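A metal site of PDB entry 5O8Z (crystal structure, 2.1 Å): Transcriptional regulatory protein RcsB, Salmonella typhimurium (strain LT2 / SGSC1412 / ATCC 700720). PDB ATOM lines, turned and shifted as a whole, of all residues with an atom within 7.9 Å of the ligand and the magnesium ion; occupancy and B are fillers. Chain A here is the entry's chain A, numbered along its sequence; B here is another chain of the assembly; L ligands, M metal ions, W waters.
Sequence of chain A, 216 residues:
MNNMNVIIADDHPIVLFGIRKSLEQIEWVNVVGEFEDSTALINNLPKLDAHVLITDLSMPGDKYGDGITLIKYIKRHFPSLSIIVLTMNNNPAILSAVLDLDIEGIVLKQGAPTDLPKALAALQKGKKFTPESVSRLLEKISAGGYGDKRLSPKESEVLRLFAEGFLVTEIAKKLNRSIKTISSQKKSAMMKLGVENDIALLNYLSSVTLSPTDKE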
ATOM      1  N   ALA A   9      20.506 -13.552 -24.475  1.00  0.00           N
ATOM      2  CA  ALA A   9      20.881 -12.616 -23.409  1.00  0.00           C
ATOM      3  C   ALA A   9      19.681 -12.118 -22.581  1.00  0.00           C
ATOM      4  O   ALA A   9      18.744 -11.588 -23.138  1.00  0.00           O
ATOM      5  CB  ALA A   9      21.610 -11.439 -23.998  1.00  0.00           C
ATOM      6  N   ASP A  10      19.763 -12.286 -21.269  1.00  0.00           N
ATOM      7  CA  ASP A  10      18.743 -11.791 -20.349  1.00  0.00           C
ATOM      8  C   ASP A  10      19.332 -11.770 -18.970  1.00  0.00           C
ATOM      9  O   ASP A  10      20.015 -12.708 -18.606  1.00  0.00           O
ATOM     10  CB  ASP A  10      17.492 -12.691 -20.369  1.00  0.00           C
ATOM     11  CG  ASP A  10      16.296 -12.045 -19.707  1.00  0.00           C
ATOM     12  OD1 ASP A  10      16.278 -11.875 -18.451  1.00  0.00           O
ATOM     13  OD2 ASP A  10      15.341 -11.668 -20.450  1.00  0.00           O
ATOM     14  N   ASP A  11      19.050 -10.742 -18.175  1.00  0.00           N
ATOM     15  CA  ASP A  11      19.579 -10.715 -16.789  1.00  0.00           C
ATOM     16  C   ASP A  11      18.906 -11.667 -15.793  1.00  0.00           C
ATOM     17  O   ASP A  11      19.324 -11.724 -14.661  1.00  0.00           O
ATOM     18  CB  ASP A  11      19.637  -9.263 -16.232  1.00  0.00           C
ATOM     19  CG  ASP A  11      18.281  -8.546 -16.225  1.00  0.00           C
ATOM     20  OD1 ASP A  11      17.548  -8.593 -17.239  1.00  0.00           O
ATOM     21  OD2 ASP A  11      17.936  -7.903 -15.208  1.00  0.00           O
ATOM     22  N   HIS A  12      17.866 -12.394 -16.200  1.00  0.00           N
ATOM     23  CA  HIS A  12      17.212 -13.388 -15.349  1.00  0.00           C
ATOM     24  C   HIS A  12      17.556 -14.820 -15.795  1.00  0.00           C
ATOM     25  O   HIS A  12      17.050 -15.244 -16.818  1.00  0.00           O
ATOM     26  CB  HIS A  12      15.693 -13.180 -15.397  1.00  0.00           C
ATOM     27  CG  HIS A  12      15.238 -11.881 -14.834  1.00  0.00           C
ATOM     28  ND1 HIS A  12      13.981 -11.356 -15.076  1.00  0.00           N
ATOM     29  CD2 HIS A  12      15.869 -10.976 -14.056  1.00  0.00           C
ATOM     30  CE1 HIS A  12      13.863 -10.199 -14.463  1.00  0.00           C
ATOM     31  NE2 HIS A  12      14.997  -9.948 -13.825  1.00  0.00           N
ATOM     32  N   VAL A  15      14.811 -17.063 -17.157  1.00  0.00           N
ATOM     33  CA  VAL A  15      14.356 -16.816 -18.529  1.00  0.00           C
ATOM     34  C   VAL A  15      15.299 -17.492 -19.528  1.00  0.00           C
ATOM     35  O   VAL A  15      14.835 -18.035 -20.519  1.00  0.00           O
ATOM     36  CB  VAL A  15      14.255 -15.284 -18.817  1.00  0.00           C
ATOM     37  CG1 VAL A  15      14.087 -14.963 -20.296  1.00  0.00           C
ATOM     38  CG2 VAL A  15      13.123 -14.679 -18.043  1.00  0.00           C
ATOM     39  N   GLU A  36      24.183 -12.553 -19.337  1.00  0.00           N
ATOM     40  CA  GLU A  36      23.307 -11.911 -18.386  1.00  0.00           C
ATOM     41  C   GLU A  36      23.518 -10.378 -18.274  1.00  0.00           C
ATOM     42  O   GLU A  36      22.813  -9.696 -17.510  1.00  0.00           O
ATOM     43  CB  GLU A  36      23.429 -12.610 -17.029  1.00  0.00           C
ATOM     44  CG  GLU A  36      23.162 -14.128 -17.084  1.00  0.00           C
ATOM     45  CD  GLU A  36      23.333 -14.833 -15.742  1.00  0.00           C
ATOM     46  OE1 GLU A  36      23.080 -14.176 -14.703  1.00  0.00           O
ATOM     47  OE2 GLU A  36      23.710 -16.045 -15.710  1.00  0.00           O
ATOM     48  N   THR A  55      17.576 -11.255 -27.472  1.00  0.00           N
ATOM     49  CA  THR A  55      18.012 -10.398 -26.364  1.00  0.00           C
ATOM     50  C   THR A  55      16.893  -9.721 -25.609  1.00  0.00           C
ATOM     51  O   THR A  55      15.891  -9.285 -26.172  1.00  0.00           O
ATOM     52  CB  THR A  55      19.010  -9.300 -26.824  1.00  0.00           C
ATOM     53  OG1 THR A  55      19.466  -8.544 -25.682  1.00  0.00           O
ATOM     54  CG2 THR A  55      18.412  -8.336 -27.839  1.00  0.00           C
ATOM     55  N   ASP A  56      17.143  -9.586 -24.321  1.00  0.00           N
ATOM     56  CA  ASP A  56      16.323  -8.807 -23.430  1.00  0.00           C
ATOM     57  C   ASP A  56      16.573  -7.316 -23.656  1.00  0.00           C
ATOM     58  O   ASP A  56      17.653  -6.908 -24.071  1.00  0.00           O
ATOM     59  CB  ASP A  56      16.749  -9.178 -22.030  1.00  0.00           C
ATOM     60  CG  ASP A  56      15.823  -8.713 -21.001  1.00  0.00           C
ATOM     61  OD1 ASP A  56      14.688  -8.317 -21.311  1.00  0.00           O
ATOM     62  OD2 ASP A  56      16.235  -8.792 -19.849  1.00  0.00           O
ATOM     63  N   LEU A  57      15.574  -6.511 -23.340  1.00  0.00           N
ATOM     64  CA  LEU A  57      15.684  -5.072 -23.493  1.00  0.00           C
ATOM     65  C   LEU A  57      16.353  -4.406 -22.286  1.00  0.00           C
ATOM     66  O   LEU A  57      17.202  -3.531 -22.478  1.00  0.00           O
ATOM     67  CB  LEU A  57      14.287  -4.504 -23.780  1.00  0.00           C
ATOM     68  CG  LEU A  57      14.074  -3.318 -24.725  1.00  0.00           C
ATOM     69  CD1 LEU A  57      14.869  -3.438 -26.028  1.00  0.00           C
ATOM     70  CD2 LEU A  57      12.587  -3.217 -25.022  1.00  0.00           C
ATOM     71  N   SER A  58      15.944  -4.770 -21.072  1.00  0.00           N
ATOM     72  CA  SER A  58      16.494  -4.203 -19.818  1.00  0.00           C
ATOM     73  C   SER A  58      17.421  -5.209 -19.179  1.00  0.00           C
ATOM     74  O   SER A  58      16.980  -6.279 -18.765  1.00  0.00           O
ATOM     75  CB  SER A  58      15.413  -3.828 -18.786  1.00  0.00           C
ATOM     76  OG  SER A  58      14.406  -3.041 -19.365  1.00  0.00           O
ATOM     77  N   MET A  59      18.703  -4.842 -19.104  1.00  0.00           N
ATOM     78  CA  MET A  59      19.753  -5.686 -18.531  1.00  0.00           C
ATOM     79  C   MET A  59      20.837  -4.739 -18.030  1.00  0.00           C
ATOM     80  O   MET A  59      21.010  -3.678 -18.617  1.00  0.00           O
ATOM     81  CB  MET A  59      20.455  -6.503 -19.623  1.00  0.00           C
ATOM     82  CG  MET A  59      19.678  -7.551 -20.341  1.00  0.00           C
ATOM     83  SD  MET A  59      20.795  -8.504 -21.400  1.00  0.00           S
ATOM     84  CE  MET A  59      21.599  -7.253 -22.396  1.00  0.00           C
ATOM     85  N   PRO A  60      21.647  -5.176 -17.064  1.00  0.00           N
ATOM     86  CA  PRO A  60      22.847  -4.395 -16.722  1.00  0.00           C
ATOM     87  C   PRO A  60      23.878  -4.307 -17.850  1.00  0.00           C
ATOM     88  O   PRO A  60      23.834  -5.087 -18.813  1.00  0.00           O
ATOM     89  CB  PRO A  60      23.450  -5.137 -15.516  1.00  0.00           C
ATOM     90  CG  PRO A  60      22.389  -6.097 -15.085  1.00  0.00           C
ATOM     91  CD  PRO A  60      21.576  -6.411 -16.283  1.00  0.00           C
ATOM     92  N   ASP A  66      21.866  -0.848 -22.582  1.00  0.00           N
ATOM     93  CA  ASP A  66      20.844  -1.801 -22.869  1.00  0.00           C
ATOM     94  C   ASP A  66      19.816  -1.093 -23.711  1.00  0.00           C
ATOM     95  O   ASP A  66      20.048   0.037 -24.161  1.00  0.00           O
ATOM     96  CB  ASP A  66      20.278  -2.390 -21.558  1.00  0.00           C
ATOM     97  CG  ASP A  66      19.498  -1.375 -20.722  1.00  0.00           C
ATOM     98  OD1 ASP A  66      19.519  -0.156 -21.006  1.00  0.00           O
ATOM     99  OD2 ASP A  66      18.839  -1.814 -19.737  1.00  0.00           O
ATOM    100  N   GLY A  67      18.697  -1.752 -23.966  1.00  0.00           N
ATOM    101  CA  GLY A  67      17.588  -1.087 -24.640  1.00  0.00           C
ATOM    102  C   GLY A  67      17.936  -0.707 -26.058  1.00  0.00           C
ATOM    103  O   GLY A  67      18.641  -1.443 -26.754  1.00  0.00           O
ATOM    104  N   VAL A  85      14.015  -9.322 -30.177  1.00  0.00           N
ATOM    105  CA  VAL A  85      13.959  -8.747 -28.840  1.00  0.00           C
ATOM    106  C   VAL A  85      12.884  -9.462 -28.076  1.00  0.00           C
ATOM    107  O   VAL A  85      11.788  -9.637 -28.585  1.00  0.00           O
ATOM    108  CB  VAL A  85      13.705  -7.238 -28.853  1.00  0.00           C
ATOM    109  CG1 VAL A  85      13.467  -6.698 -27.438  1.00  0.00           C
ATOM    110  CG2 VAL A  85      14.895  -6.562 -29.490  1.00  0.00           C
ATOM    111  N   LEU A  86      13.236  -9.919 -26.873  1.00  0.00           N
ATOM    112  CA  LEU A  86      12.333 -10.648 -26.006  1.00  0.00           C
ATOM    113  C   LEU A  86      12.234  -9.832 -24.735  1.00  0.00           C
ATOM    114  O   LEU A  86      13.223  -9.714 -24.026  1.00  0.00           O
ATOM    115  CB  LEU A  86      12.859 -12.054 -25.715  1.00  0.00           C
ATOM    116  CG  LEU A  86      12.124 -12.844 -24.626  1.00  0.00           C
ATOM    117  CD1 LEU A  86      10.655 -13.079 -24.979  1.00  0.00           C
ATOM    118  CD2 LEU A  86      12.811 -14.176 -24.389  1.00  0.00           C
ATOM    119  N   THR A  87      11.048  -9.288 -24.440  1.00  0.00           N
ATOM    120  CA  THR A  87      10.905  -8.294 -23.379  1.00  0.00           C
ATOM    121  C   THR A  87       9.576  -8.320 -22.691  1.00  0.00           C
ATOM    122  O   THR A  87       8.559  -8.635 -23.304  1.00  0.00           O
ATOM    123  CB  THR A  87      11.139  -6.860 -23.907  1.00  0.00           C
ATOM    124  OG1 THR A  87      11.209  -5.956 -22.801  1.00  0.00           O
ATOM    125  CG2 THR A  87      10.042  -6.390 -24.902  1.00  0.00           C
ATOM    126  N   MET A  88       9.622  -8.007 -21.405  1.00  0.00           N
ATOM    127  CA  MET A  88       8.433  -7.737 -20.619  1.00  0.00           C
ATOM    128  C   MET A  88       7.940  -6.297 -20.760  1.00  0.00           C
ATOM    129  O   MET A  88       6.834  -6.005 -20.334  1.00  0.00           O
ATOM    130  CB  MET A  88       8.681  -8.033 -19.137  1.00  0.00           C
ATOM    131  CG  MET A  88       9.566  -7.051 -18.382  1.00  0.00           C
ATOM    132  SD  MET A  88       9.895  -7.739 -16.754  1.00  0.00           S
ATOM    133  CE  MET A  88      11.409  -8.645 -17.026  1.00  0.00           C
ATOM    134  N   ASN A  89       8.748  -5.396 -21.339  1.00  0.00           N
ATOM    135  CA  ASN A  89       8.283  -4.021 -21.547  1.00  0.00           C
ATOM    136  C   ASN A  89       6.991  -3.983 -22.359  1.00  0.00           C
ATOM    137  O   ASN A  89       6.933  -4.567 -23.443  1.00  0.00           O
ATOM    138  CB  ASN A  89       9.334  -3.141 -22.232  1.00  0.00           C
ATOM    139  CG  ASN A  89       9.016  -1.652 -22.098  1.00  0.00           C
ATOM    140  OD1 ASN A  89       8.170  -1.098 -22.834  1.00  0.00           O
ATOM    141  ND2 ASN A  89       9.680  -0.994 -21.152  1.00  0.00           N
ATOM    142  N   VAL A 107       9.263 -10.521 -29.349  1.00  0.00           N
ATOM    143  CA  VAL A 107       8.453 -11.440 -28.590  1.00  0.00           C
ATOM    144  C   VAL A 107       8.243 -10.776 -27.223  1.00  0.00           C
ATOM    145  O   VAL A 107       9.174 -10.254 -26.623  1.00  0.00           O
ATOM    146  CB  VAL A 107       9.132 -12.837 -28.485  1.00  0.00           C
ATOM    147  CG1 VAL A 107       8.208 -13.849 -27.819  1.00  0.00           C
ATOM    148  CG2 VAL A 107       9.523 -13.359 -29.865  1.00  0.00           C
ATOM    149  N   LEU A 108       6.998 -10.765 -26.764  1.00  0.00           N
ATOM    150  CA  LEU A 108       6.692 -10.245 -25.443  1.00  0.00           C
ATOM    151  C   LEU A 108       6.677 -11.416 -24.454  1.00  0.00           C
ATOM    152  O   LEU A 108       6.135 -12.489 -24.754  1.00  0.00           O
ATOM    153  CB  LEU A 108       5.344  -9.526 -25.447  1.00  0.00           C
ATOM    154  CG  LEU A 108       5.148  -8.329 -26.404  1.00  0.00           C
ATOM    155  CD1 LEU A 108       3.724  -7.811 -26.298  1.00  0.00           C
ATOM    156  CD2 LEU A 108       6.153  -7.204 -26.179  1.00  0.00           C
ATOM    157  N   LYS A 109       7.256 -11.206 -23.257  1.00  0.00           N
ATOM    158  CA  LYS A 109       7.278 -12.218 -22.194  1.00  0.00           C
ATOM    159  C   LYS A 109       5.895 -12.551 -21.644  1.00  0.00           C
ATOM    160  O   LYS A 109       5.727 -13.576 -20.985  1.00  0.00           O
ATOM    161  CB  LYS A 109       8.199 -11.784 -21.043  1.00  0.00           C
ATOM    162  CG  LYS A 109       9.667 -11.695 -21.410  1.00  0.00           C
ATOM    163  CD  LYS A 109      10.544 -11.203 -20.262  1.00  0.00           C
ATOM    164  CE  LYS A 109      12.007 -11.418 -20.582  1.00  0.00           C
ATOM    165  NZ  LYS A 109      12.898 -10.923 -19.495  1.00  0.00           N
ATOM    166  N   GLN A 110       4.915 -11.687 -21.901  1.00  0.00           N
ATOM    167  CA  GLN A 110       3.504 -11.951 -21.576  1.00  0.00           C
ATOM    168  C   GLN A 110       2.826 -12.866 -22.631  1.00  0.00           C
ATOM    169  O   GLN A 110       1.808 -13.465 -22.341  1.00  0.00           O
ATOM    170  CB  GLN A 110       2.720 -10.650 -21.493  1.00  0.00           C
ATOM    171  CG  GLN A 110       3.187  -9.670 -20.394  1.00  0.00           C
ATOM    172  CD  GLN A 110       4.379  -8.785 -20.771  1.00  0.00           C
ATOM    173  OE1 GLN A 110       5.070  -9.006 -21.776  1.00  0.00           O
ATOM    174  NE2 GLN A 110       4.662  -7.825 -19.915  1.00  0.00           N
ATOM    175  N   ARG A 160      12.145   5.162 -19.551  1.00  0.00           N
ATOM    176  CA  ARG A 160      12.226   3.736 -19.196  1.00  0.00           C
ATOM    177  C   ARG A 160      13.098   3.512 -17.976  1.00  0.00           C
ATOM    178  O   ARG A 160      12.673   2.878 -17.003  1.00  0.00           O
ATOM    179  CB  ARG A 160      12.772   2.892 -20.353  1.00  0.00           C
ATOM    180  CG  ARG A 160      12.835   1.386 -20.029  1.00  0.00           C
ATOM    181  CD  ARG A 160      13.267   0.537 -21.214  1.00  0.00           C
ATOM    182  NE  ARG A 160      14.622   0.873 -21.651  1.00  0.00           N
ATOM    183  CZ  ARG A 160      15.762   0.417 -21.122  1.00  0.00           C
ATOM    184  NH1 ARG A 160      15.780  -0.423 -20.092  1.00  0.00           N
ATOM    185  NH2 ARG A 160      16.914   0.824 -21.625  1.00  0.00           N
ATOM    186  N   HIS B  12       4.321 -14.898 -16.972  1.00  0.00           N
ATOM    187  CA  HIS B  12       5.155 -14.980 -18.157  1.00  0.00           C
ATOM    188  C   HIS B  12       5.421 -16.442 -18.496  1.00  0.00           C
ATOM    189  O   HIS B  12       6.171 -17.091 -17.774  1.00  0.00           O
ATOM    190  CB  HIS B  12       6.494 -14.287 -17.903  1.00  0.00           C
ATOM    191  CG  HIS B  12       6.384 -12.818 -17.711  1.00  0.00           C
ATOM    192  ND1 HIS B  12       7.371 -12.073 -17.107  1.00  0.00           N
ATOM    193  CD2 HIS B  12       5.414 -11.939 -18.059  1.00  0.00           C
ATOM    194  CE1 HIS B  12       7.025 -10.801 -17.090  1.00  0.00           C
ATOM    195  NE2 HIS B  12       5.844 -10.698 -17.659  1.00  0.00           N
ATOM    196  N   MET B  88      10.973 -10.952  -9.592  1.00  0.00           N
ATOM    197  CA  MET B  88      11.908  -9.929 -10.037  1.00  0.00           C
ATOM    198  C   MET B  88      11.836  -8.660  -9.193  1.00  0.00           C
ATOM    199  O   MET B  88      12.594  -7.737  -9.454  1.00  0.00           O
ATOM    200  CB  MET B  88      11.627  -9.556 -11.502  1.00  0.00           C
ATOM    201  CG  MET B  88      10.353  -8.743 -11.711  1.00  0.00           C
ATOM    202  SD  MET B  88      10.019  -8.460 -13.456  1.00  0.00           S
ATOM    203  CE  MET B  88       9.002  -9.891 -13.813  1.00  0.00           C
ATOM    204  N   GLN B 110      16.567 -12.069 -10.611  1.00  0.00           N
ATOM    205  CA  GLN B 110      17.907 -11.464 -10.804  1.00  0.00           C
ATOM    206  C   GLN B 110      19.017 -12.232 -10.084  1.00  0.00           C
ATOM    207  O   GLN B 110      20.143 -11.779 -10.110  1.00  0.00           O
ATOM    208  CB  GLN B 110      18.016 -10.019 -10.252  1.00  0.00           C
ATOM    209  CG  GLN B 110      16.943  -9.044 -10.666  1.00  0.00           C
ATOM    210  CD  GLN B 110      15.724  -9.062  -9.768  1.00  0.00           C
ATOM    211  OE1 GLN B 110      15.231 -10.125  -9.369  1.00  0.00           O
ATOM    212  NE2 GLN B 110      15.209  -7.893  -9.496  1.00  0.00           N
HETATM  213 BE1  LIG L   1      13.492  -7.500 -20.230  1.00  0.00          BE
HETATM  214  F1  LIG L   1      14.117  -7.082 -18.929  1.00  0.00           F
HETATM  215  F2  LIG L   1      13.345  -6.275 -21.080  1.00  0.00           F
HETATM  216  F3  LIG L   1      12.219  -8.294 -20.193  1.00  0.00           F
HETATM  217 MG    MG M   1      15.785  -7.754 -18.000  1.00  0.00          MG
HETATM  218  O   HOH W   1      11.907  -4.056 -20.067  1.00  0.00           O
HETATM  219  O   HOH W   2      15.436  -6.881 -16.359  1.00  0.00           O
HETATM  220  O   HOH W   3      14.861  -9.616 -17.610  1.00  0.00           O
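Water W3 lies within hydrogen-bond range of the side-chain carboxylate of Asp 10 (2.8 Å), the side-chain amino group of Lys 109 (3.0 Å) and a ring nitrogen (ND1) of His 12 of chain A (3.2 Å).
Water W1 lies within hydrogen-bond range of OG of Ser 58, F2 of the ligand and OG1 of Thr 87.
Hydrophobic or aromatic side chains within 4 Å of the ligand: Leu 57 and Met 88 of chain A.
Within 4 Å of the ligand: Asp 56, Leu 57, Ser 58, Thr 87, Met 88 of chain A and Lys 109.
BE1 of the ligand is bound by OD1 of Asp 56.
A fluorine (F2) of the ligand sits at hydrogen-bond distance from the backbone NH (N) of Ser 58, 3.0 Å away.
The side-chain hydroxyl of Thr 87 is in hydrogen-bond range of a fluorine (F2) of the ligand (2.8 Å).
The side-chain amino group of Lys 109 is in hydrogen-bond range of a fluorine (F3) of the ligand (2.8 Å).
N of Met 88 of chain A is in hydrogen-bond range of F3 of the ligand (2.9 Å).
The backbone NH (N) of Leu 57 lies within hydrogen-bond range of a fluorine (F2) of the ligand (3.2 Å).
The magnesium ion is bound by water W2 (1.9 Å), F1 of the ligand (2.0 Å), O of Ser 58 (2.0 Å), OD1 of Asp 11 (2.1 Å), water W3 (2.1 Å) and OD2 of Asp 56 (2.2 Å).
The magnesium ion has six donor atoms within binding distance.
Within 4 Å of the magnesium ion: Asp 11, Asp 56 and Ser 58.
The nearest printed residue that does not touch the magnesium ion is Asp 10 (4.2 Å).
OD1 of Asp 56 lies close to NZ of Lys 109 (3.6 Å).
The backbone NH of Asp 56 is in hydrogen-bond range of the backbone carbonyl oxygen of Ala 9 (2.8 Å).
NH1 of Arg 160 is in hydrogen-bond range of OG of Ser 58 (3.0 Å).
N of Lys 109 lies within hydrogen-bond range of O of Thr 87, 2.9 Å away.
The side-chain hydroxyl (OG1) of Thr 87 sits at hydrogen-bond distance from the backbone NH (N) of Asn 89 (2.9 Å).
N of Thr 87 lies within hydrogen-bond range of O of Val 107.
The side-chain amino group (NZ) of Lys 109 lies within salt-bridge range of the side-chain carboxylate (OD2) of Asp 10.
The backbone NH (N) of Gly 67 sits at hydrogen-bond distance from the backbone carbonyl oxygen (O) of Leu 57 (2.8 Å).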
